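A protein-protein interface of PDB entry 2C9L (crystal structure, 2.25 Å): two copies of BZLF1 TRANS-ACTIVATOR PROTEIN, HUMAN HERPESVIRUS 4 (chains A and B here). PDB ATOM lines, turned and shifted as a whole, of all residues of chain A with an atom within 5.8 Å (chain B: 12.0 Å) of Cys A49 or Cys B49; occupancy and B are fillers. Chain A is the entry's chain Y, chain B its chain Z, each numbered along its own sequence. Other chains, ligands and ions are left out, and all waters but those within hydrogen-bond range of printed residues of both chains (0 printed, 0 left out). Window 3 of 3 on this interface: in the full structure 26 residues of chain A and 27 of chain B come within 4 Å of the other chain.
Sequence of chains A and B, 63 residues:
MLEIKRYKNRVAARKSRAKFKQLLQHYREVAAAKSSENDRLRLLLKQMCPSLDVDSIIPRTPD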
ATOM      1  N   LEU A  44      -0.362  28.437   3.603  1.00  0.00           N
ATOM      2  CA  LEU A  44       0.228  28.113   2.307  1.00  0.00           C
ATOM      3  C   LEU A  44       0.339  26.600   2.156  1.00  0.00           C
ATOM      4  O   LEU A  44       0.052  26.049   1.099  1.00  0.00           O
ATOM      5  CB  LEU A  44       1.621  28.731   2.174  1.00  0.00           C
ATOM      6  CG  LEU A  44       2.394  28.345   0.909  1.00  0.00           C
ATOM      7  CD1 LEU A  44       1.575  28.688  -0.322  1.00  0.00           C
ATOM      8  CD2 LEU A  44       3.730  29.075   0.881  1.00  0.00           C
ATOM      9  N   LEU A  45       0.754  25.931   3.226  1.00  0.00           N
ATOM     10  CA  LEU A  45       0.902  24.484   3.201  1.00  0.00           C
ATOM     11  C   LEU A  45      -0.454  23.831   2.983  1.00  0.00           C
ATOM     12  O   LEU A  45      -0.561  22.788   2.338  1.00  0.00           O
ATOM     13  CB  LEU A  45       1.505  23.998   4.516  1.00  0.00           C
ATOM     14  CG  LEU A  45       1.803  22.505   4.654  1.00  0.00           C
ATOM     15  CD1 LEU A  45       2.682  22.030   3.497  1.00  0.00           C
ATOM     16  CD2 LEU A  45       2.492  22.260   5.991  1.00  0.00           C
ATOM     17  N   LYS A  46      -1.489  24.459   3.526  1.00  0.00           N
ATOM     18  CA  LYS A  46      -2.841  23.950   3.394  1.00  0.00           C
ATOM     19  C   LYS A  46      -3.319  24.151   1.952  1.00  0.00           C
ATOM     20  O   LYS A  46      -3.970  23.279   1.388  1.00  0.00           O
ATOM     21  CB  LYS A  46      -3.772  24.673   4.369  1.00  0.00           C
ATOM     22  CG  LYS A  46      -5.093  23.961   4.602  1.00  0.00           C
ATOM     23  CD  LYS A  46      -4.879  22.611   5.273  1.00  0.00           C
ATOM     24  CE  LYS A  46      -6.200  21.905   5.533  1.00  0.00           C
ATOM     25  NZ  LYS A  46      -6.028  20.563   6.168  1.00  0.00           N
ATOM     26  N   GLN A  47      -2.984  25.293   1.356  1.00  0.00           N
ATOM     27  CA  GLN A  47      -3.382  25.571  -0.022  1.00  0.00           C
ATOM     28  C   GLN A  47      -2.758  24.557  -0.973  1.00  0.00           C
ATOM     29  O   GLN A  47      -3.435  24.031  -1.853  1.00  0.00           O
ATOM     30  CB  GLN A  47      -2.952  26.978  -0.455  1.00  0.00           C
ATOM     31  CG  GLN A  47      -3.603  28.113   0.307  1.00  0.00           C
ATOM     32  CD  GLN A  47      -3.370  29.462  -0.348  1.00  0.00           C
ATOM     33  OE1 GLN A  47      -2.274  29.754  -0.827  1.00  0.00           O
ATOM     34  NE2 GLN A  47      -4.403  30.296  -0.360  1.00  0.00           N
ATOM     35  N   MET A  48      -1.467  24.287  -0.788  1.00  0.00           N
ATOM     36  CA  MET A  48      -0.746  23.341  -1.634  1.00  0.00           C
ATOM     37  C   MET A  48      -1.114  21.891  -1.351  1.00  0.00           C
ATOM     38  O   MET A  48      -1.184  21.077  -2.269  1.00  0.00           O
ATOM     39  CB  MET A  48       0.765  23.517  -1.458  1.00  0.00           C
ATOM     40  CG  MET A  48       1.251  24.931  -1.709  1.00  0.00           C
ATOM     41  SD  MET A  48       0.635  25.578  -3.269  1.00  0.00           S
ATOM     42  CE  MET A  48       1.770  24.817  -4.426  1.00  0.00           C
ATOM     43  N   CYS A  49      -1.339  21.567  -0.081  1.00  0.00           N
ATOM     44  CA  CYS A  49      -1.694  20.205   0.311  1.00  0.00           C
ATOM     45  C   CYS A  49      -3.024  20.209   1.059  1.00  0.00           C
ATOM     46  O   CYS A  49      -3.081  19.959   2.267  1.00  0.00           O
ATOM     47  CB  CYS A  49      -0.600  19.606   1.193  1.00  0.00           C
ATOM     48  SG  CYS A  49       1.037  19.592   0.426  1.00  0.00           S
ATOM     49  N   PRO A  50      -4.117  20.497   0.339  1.00  0.00           N
ATOM     50  CA  PRO A  50      -5.473  20.551   0.886  1.00  0.00           C
ATOM     51  C   PRO A  50      -5.852  19.325   1.709  1.00  0.00           C
ATOM     52  O   PRO A  50      -6.714  19.399   2.583  1.00  0.00           O
ATOM     53  CB  PRO A  50      -6.336  20.693  -0.366  1.00  0.00           C
ATOM     54  CG  PRO A  50      -5.458  21.472  -1.285  1.00  0.00           C
ATOM     55  CD  PRO A  50      -4.129  20.779  -1.109  1.00  0.00           C
ATOM     56  N   SER A  51      -5.198  18.203   1.435  1.00  0.00           N
ATOM     57  CA  SER A  51      -5.493  16.957   2.135  1.00  0.00           C
ATOM     58  C   SER A  51      -4.626  16.689   3.361  1.00  0.00           C
ATOM     59  O   SER A  51      -4.695  15.608   3.945  1.00  0.00           O
ATOM     60  CB  SER A  51      -5.368  15.784   1.158  1.00  0.00           C
ATOM     61  OG  SER A  51      -4.143  15.850   0.442  1.00  0.00           O
ATOM     62  N   LEU A  52      -3.825  17.670   3.762  1.00  0.00           N
ATOM     63  CA  LEU A  52      -2.945  17.499   4.913  1.00  0.00           C
ATOM     64  C   LEU A  52      -3.433  18.231   6.168  1.00  0.00           C
ATOM     65  O   LEU A  52      -3.766  19.418   6.119  1.00  0.00           O
ATOM     66  CB  LEU A  52      -1.533  17.973   4.547  1.00  0.00           C
ATOM     67  CG  LEU A  52      -0.413  17.736   5.562  1.00  0.00           C
ATOM     68  CD1 LEU A  52      -0.271  16.249   5.840  1.00  0.00           C
ATOM     69  CD2 LEU A  52       0.887  18.304   5.014  1.00  0.00           C
ATOM     70  N   ASP A  53      -3.475  17.516   7.292  1.00  0.00           N
ATOM     71  CA  ASP A  53      -3.910  18.096   8.562  1.00  0.00           C
ATOM     72  C   ASP A  53      -2.700  18.690   9.278  1.00  0.00           C
ATOM     73  O   ASP A  53      -2.102  18.051  10.145  1.00  0.00           O
ATOM     74  CB  ASP A  53      -4.551  17.028   9.453  1.00  0.00           C
ATOM     75  CG  ASP A  53      -5.269  17.625  10.650  1.00  0.00           C
ATOM     76  OD1 ASP A  53      -4.816  18.678  11.144  1.00  0.00           O
ATOM     77  OD2 ASP A  53      -6.276  17.042  11.104  1.00  0.00           O
ATOM     78  N   ARG B  40      10.251  24.130  11.238  1.00  0.00           N
ATOM     79  CA  ARG B  40       9.697  22.802  10.998  1.00  0.00           C
ATOM     80  C   ARG B  40       8.652  22.871   9.883  1.00  0.00           C
ATOM     81  O   ARG B  40       8.513  21.939   9.092  1.00  0.00           O
ATOM     82  CB  ARG B  40       9.061  22.235  12.271  1.00  0.00           C
ATOM     83  CG  ARG B  40      10.038  22.036  13.424  1.00  0.00           C
ATOM     84  CD  ARG B  40       9.573  20.932  14.372  1.00  0.00           C
ATOM     85  NE  ARG B  40       8.337  21.255  15.084  1.00  0.00           N
ATOM     86  CZ  ARG B  40       8.253  22.113  16.098  1.00  0.00           C
ATOM     87  NH1 ARG B  40       9.335  22.747  16.530  1.00  0.00           N
ATOM     88  NH2 ARG B  40       7.085  22.332  16.688  1.00  0.00           N
ATOM     89  N   LEU B  41       7.923  23.982   9.824  1.00  0.00           N
ATOM     90  CA  LEU B  41       6.907  24.169   8.794  1.00  0.00           C
ATOM     91  C   LEU B  41       7.575  24.350   7.440  1.00  0.00           C
ATOM     92  O   LEU B  41       7.123  23.791   6.445  1.00  0.00           O
ATOM     93  CB  LEU B  41       6.038  25.391   9.108  1.00  0.00           C
ATOM     94  CG  LEU B  41       5.038  25.238  10.253  1.00  0.00           C
ATOM     95  CD1 LEU B  41       4.536  26.605  10.688  1.00  0.00           C
ATOM     96  CD2 LEU B  41       3.887  24.346   9.808  1.00  0.00           C
ATOM     97  N   ARG B  42       8.651  25.135   7.409  1.00  0.00           N
ATOM     98  CA  ARG B  42       9.388  25.381   6.171  1.00  0.00           C
ATOM     99  C   ARG B  42      10.003  24.106   5.615  1.00  0.00           C
ATOM    100  O   ARG B  42      10.111  23.937   4.401  1.00  0.00           O
ATOM    101  CB  ARG B  42      10.499  26.402   6.402  1.00  0.00           C
ATOM    102  CG  ARG B  42      10.012  27.824   6.494  1.00  0.00           C
ATOM    103  CD  ARG B  42      11.137  28.759   6.893  1.00  0.00           C
ATOM    104  NE  ARG B  42      10.673  30.140   6.945  1.00  0.00           N
ATOM    105  CZ  ARG B  42      10.378  30.868   5.875  1.00  0.00           C
ATOM    106  NH1 ARG B  42      10.509  30.350   4.659  1.00  0.00           N
ATOM    107  NH2 ARG B  42       9.935  32.108   6.024  1.00  0.00           N
ATOM    108  N   LEU B  43      10.415  23.216   6.509  1.00  0.00           N
ATOM    109  CA  LEU B  43      11.016  21.963   6.085  1.00  0.00           C
ATOM    110  C   LEU B  43       9.926  21.039   5.562  1.00  0.00           C
ATOM    111  O   LEU B  43      10.101  20.387   4.537  1.00  0.00           O
ATOM    112  CB  LEU B  43      11.756  21.296   7.250  1.00  0.00           C
ATOM    113  CG  LEU B  43      12.525  20.017   6.894  1.00  0.00           C
ATOM    114  CD1 LEU B  43      13.552  20.321   5.813  1.00  0.00           C
ATOM    115  CD2 LEU B  43      13.208  19.460   8.133  1.00  0.00           C
ATOM    116  N   LEU B  44       8.796  20.999   6.262  1.00  0.00           N
ATOM    117  CA  LEU B  44       7.680  20.152   5.855  1.00  0.00           C
ATOM    118  C   LEU B  44       7.191  20.537   4.462  1.00  0.00           C
ATOM    119  O   LEU B  44       6.887  19.675   3.643  1.00  0.00           O
ATOM    120  CB  LEU B  44       6.524  20.268   6.852  1.00  0.00           C
ATOM    121  CG  LEU B  44       5.352  19.310   6.611  1.00  0.00           C
ATOM    122  CD1 LEU B  44       5.864  17.879   6.623  1.00  0.00           C
ATOM    123  CD2 LEU B  44       4.285  19.497   7.679  1.00  0.00           C
ATOM    124  N   LEU B  45       7.124  21.835   4.195  1.00  0.00           N
ATOM    125  CA  LEU B  45       6.661  22.319   2.899  1.00  0.00           C
ATOM    126  C   LEU B  45       7.672  21.979   1.807  1.00  0.00           C
ATOM    127  O   LEU B  45       7.302  21.685   0.671  1.00  0.00           O
ATOM    128  CB  LEU B  45       6.430  23.831   2.968  1.00  0.00           C
ATOM    129  CG  LEU B  45       5.757  24.560   1.800  1.00  0.00           C
ATOM    130  CD1 LEU B  45       4.444  23.887   1.418  1.00  0.00           C
ATOM    131  CD2 LEU B  45       5.508  26.001   2.212  1.00  0.00           C
ATOM    132  N   LYS B  46       8.950  22.011   2.158  1.00  0.00           N
ATOM    133  CA  LYS B  46       9.999  21.692   1.201  1.00  0.00           C
ATOM    134  C   LYS B  46       9.887  20.223   0.809  1.00  0.00           C
ATOM    135  O   LYS B  46       9.895  19.884  -0.374  1.00  0.00           O
ATOM    136  CB  LYS B  46      11.374  21.957   1.815  1.00  0.00           C
ATOM    137  CG  LYS B  46      12.529  21.872   0.828  1.00  0.00           C
ATOM    138  CD  LYS B  46      12.445  22.976  -0.218  1.00  0.00           C
ATOM    139  CE  LYS B  46      13.618  22.916  -1.185  1.00  0.00           C
ATOM    140  NZ  LYS B  46      13.541  23.983  -2.221  1.00  0.00           N
ATOM    141  N   GLN B  47       9.768  19.353   1.807  1.00  0.00           N
ATOM    142  CA  GLN B  47       9.665  17.921   1.563  1.00  0.00           C
ATOM    143  C   GLN B  47       8.290  17.476   1.070  1.00  0.00           C
ATOM    144  O   GLN B  47       8.095  16.307   0.739  1.00  0.00           O
ATOM    145  CB  GLN B  47      10.062  17.139   2.824  1.00  0.00           C
ATOM    146  CG  GLN B  47       9.303  17.510   4.088  1.00  0.00           C
ATOM    147  CD  GLN B  47       9.948  16.938   5.344  1.00  0.00           C
ATOM    148  OE1 GLN B  47      10.141  15.728   5.464  1.00  0.00           O
ATOM    149  NE2 GLN B  47      10.283  17.811   6.287  1.00  0.00           N
ATOM    150  N   MET B  48       7.341  18.405   1.021  1.00  0.00           N
ATOM    151  CA  MET B  48       6.000  18.093   0.535  1.00  0.00           C
ATOM    152  C   MET B  48       5.818  18.700  -0.851  1.00  0.00           C
ATOM    153  O   MET B  48       5.128  18.144  -1.702  1.00  0.00           O
ATOM    154  CB  MET B  48       4.933  18.642   1.485  1.00  0.00           C
ATOM    155  CG  MET B  48       4.844  17.905   2.810  1.00  0.00           C
ATOM    156  SD  MET B  48       4.585  16.136   2.598  1.00  0.00           S
ATOM    157  CE  MET B  48       2.806  16.068   2.421  1.00  0.00           C
ATOM    158  N   CYS B  49       6.446  19.849  -1.066  1.00  0.00           N
ATOM    159  CA  CYS B  49       6.382  20.544  -2.346  1.00  0.00           C
ATOM    160  C   CYS B  49       7.801  20.999  -2.680  1.00  0.00           C
ATOM    161  O   CYS B  49       8.111  22.190  -2.651  1.00  0.00           O
ATOM    162  CB  CYS B  49       5.439  21.746  -2.242  1.00  0.00           C
ATOM    163  SG  CYS B  49       3.755  21.317  -1.710  1.00  0.00           S
ATOM    164  N   PRO B  50       8.685  20.037  -3.000  1.00  0.00           N
ATOM    165  CA  PRO B  50      10.095  20.245  -3.347  1.00  0.00           C
ATOM    166  C   PRO B  50      10.394  21.363  -4.342  1.00  0.00           C
ATOM    167  O   PRO B  50      11.342  22.124  -4.153  1.00  0.00           O
ATOM    168  CB  PRO B  50      10.518  18.878  -3.876  1.00  0.00           C
ATOM    169  CG  PRO B  50       9.692  17.944  -3.067  1.00  0.00           C
ATOM    170  CD  PRO B  50       8.337  18.609  -3.116  1.00  0.00           C
ATOM    171  N   SER B  51       9.593  21.461  -5.397  1.00  0.00           N
ATOM    172  CA  SER B  51       9.809  22.483  -6.415  1.00  0.00           C
ATOM    173  C   SER B  51       9.063  23.785  -6.140  1.00  0.00           C
ATOM    174  O   SER B  51       8.387  24.319  -7.020  1.00  0.00           O
ATOM    175  CB  SER B  51       9.409  21.946  -7.792  1.00  0.00           C
ATOM    176  OG  SER B  51       8.033  21.609  -7.829  1.00  0.00           O
ATOM    177  N   LEU B  52       9.188  24.296  -4.921  1.00  0.00           N
ATOM    178  CA  LEU B  52       8.531  25.543  -4.546  1.00  0.00           C
ATOM    179  C   LEU B  52       9.474  26.437  -3.752  1.00  0.00           C
ATOM    180  O   LEU B  52      10.021  26.021  -2.730  1.00  0.00           O
ATOM    181  CB  LEU B  52       7.279  25.264  -3.710  1.00  0.00           C
ATOM    182  CG  LEU B  52       6.604  26.505  -3.115  1.00  0.00           C
ATOM    183  CD1 LEU B  52       6.221  27.468  -4.229  1.00  0.00           C
ATOM    184  CD2 LEU B  52       5.380  26.094  -2.314  1.00  0.00           C
ATOM    185  N   ASP B  53       9.664  27.664  -4.226  1.00  0.00           N
ATOM    186  CA  ASP B  53      10.539  28.603  -3.539  1.00  0.00           C
ATOM    187  C   ASP B  53       9.716  29.375  -2.513  1.00  0.00           C
ATOM    188  O   ASP B  53       9.227  30.473  -2.786  1.00  0.00           O
ATOM    189  CB  ASP B  53      11.180  29.570  -4.537  1.00  0.00           C
ATOM    190  CG  ASP B  53      12.358  30.318  -3.942  1.00  0.00           C
ATOM    191  OD1 ASP B  53      12.173  31.005  -2.918  1.00  0.00           O
ATOM    192  OD2 ASP B  53      13.472  30.216  -4.500  1.00  0.00           O
ATOM    193  N   VAL B  54       9.566  28.781  -1.334  1.00  0.00           N
ATOM    194  CA  VAL B  54       8.799  29.375  -0.247  1.00  0.00           C
ATOM    195  C   VAL B  54       9.406  30.684   0.248  1.00  0.00           C
ATOM    196  O   VAL B  54       8.683  31.612   0.611  1.00  0.00           O
ATOM    197  CB  VAL B  54       8.695  28.401   0.944  1.00  0.00           C
ATOM    198  CG1 VAL B  54       7.837  29.004   2.042  1.00  0.00           C
ATOM    199  CG2 VAL B  54       8.113  27.076   0.477  1.00  0.00           C
ATOM    200  N   ASP B  55      10.732  30.753   0.259  1.00  0.00           N
ATOM    201  CA  ASP B  55      11.434  31.947   0.715  1.00  0.00           C
ATOM    202  C   ASP B  55      11.089  33.165  -0.134  1.00  0.00           C
ATOM    203  O   ASP B  55      11.180  34.299   0.332  1.00  0.00           O
ATOM    204  CB  ASP B  55      12.944  31.709   0.694  1.00  0.00           C
ATOM    205  CG  ASP B  55      13.344  30.473   1.475  1.00  0.00           C
ATOM    206  OD1 ASP B  55      12.968  30.373   2.661  1.00  0.00           O
ATOM    207  OD2 ASP B  55      14.036  29.602   0.905  1.00  0.00           O
ATOM    208  N   SER B  56      10.695  32.928  -1.381  1.00  0.00           N
ATOM    209  CA  SER B  56      10.332  34.015  -2.286  1.00  0.00           C
ATOM    210  C   SER B  56       8.874  34.405  -2.084  1.00  0.00           C
ATOM    211  O   SER B  56       8.405  35.402  -2.634  1.00  0.00           O
ATOM    212  CB  SER B  56      10.554  33.596  -3.741  1.00  0.00           C
ATOM    213  OG  SER B  56      11.928  33.372  -4.004  1.00  0.00           O
ATOM    214  N   ILE B  57       8.163  33.609  -1.294  1.00  0.00           N
ATOM    215  CA  ILE B  57       6.756  33.862  -1.004  1.00  0.00           C
ATOM    216  C   ILE B  57       6.635  34.398   0.417  1.00  0.00           C
ATOM    217  O   ILE B  57       5.882  35.333   0.686  1.00  0.00           O
ATOM    218  CB  ILE B  57       5.923  32.570  -1.114  1.00  0.00           C
ATOM    219  CG1 ILE B  57       6.099  31.956  -2.508  1.00  0.00           C
ATOM    220  CG2 ILE B  57       4.457  32.873  -0.835  1.00  0.00           C
ATOM    221  CD1 ILE B  57       5.384  30.626  -2.693  1.00  0.00           C
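Cys A49 touches just one residue of chain B: Cys B49 (3.9 Å). Printed residues of chain A within 4 Å of Cys B49: Met A48 and Cys A49. Of the printed residues of chain B, Leu A45 touches Leu B44 (3.7 Å) and Leu B45 (3.3 Å). Printed residues of chain B within 4 Å of Met A48: Cys B49. No residue of chain B comes within 4 Å of Pro A50. No residue of chain B comes within 4 Å of Ser A51. Of chain B, only Met B48 comes within 4 Å of Leu A52. Printed residues of chain A within 4 Å of Met B48: Leu A52. Printed residues of chain A within 4 Å of Leu B45: Leu A44 (3.8 Å) and Leu A45 (3.3 Å). Printed residues of chain A within 4 Å of Leu B44: Leu A45 (3.7 Å). The nearest printed residue of chain B that does not touch Leu A44 is Ile B57 (4.2 Å).
Printed residues of chain A that touch a printed residue of chain B: Leu A44, Leu A45, Met A48, Cys A49 and Leu A52. Hydrophobic or aromatic side chains of chain A that line the printed part of chain B: Leu A44, Leu A45, Met A48 and Leu A52. Of the 18 printed residues of chain B, 4 touch a printed residue of chain A.
Leu A44 touches Leu B45. Leu A45 touches Leu B44. Leu A45 touches Leu B45 (CD1 to CD1, 3.3 Å). Met A48 touches Cys B49. SG of Cys B49 touches SG of Cys A49, 3.9 Å away. CD2 of Leu A52 touches CE of Met B48, 3.9 Å away.
O of Leu A52 sits at hydrogen-bond distance from NZ of Lys A46, at 2.5 Å.
Leu A44 touches Leu B45, and with the chains exchanged Leu A45 touches Leu B44. Met A48 touches Cys B49, but with the chains exchanged Cys A49 does not touch Met B48 (4.1 Å). Cys B49 touches its own counterpart, Cys A49. Leu A52 touches Met B48, but with the chains exchanged Met A48 does not touch Leu B52 (4.3 Å). Of the 6 pairs that touch across the chains among the printed residues, 4 have their exchanged pair printed and touching as well.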
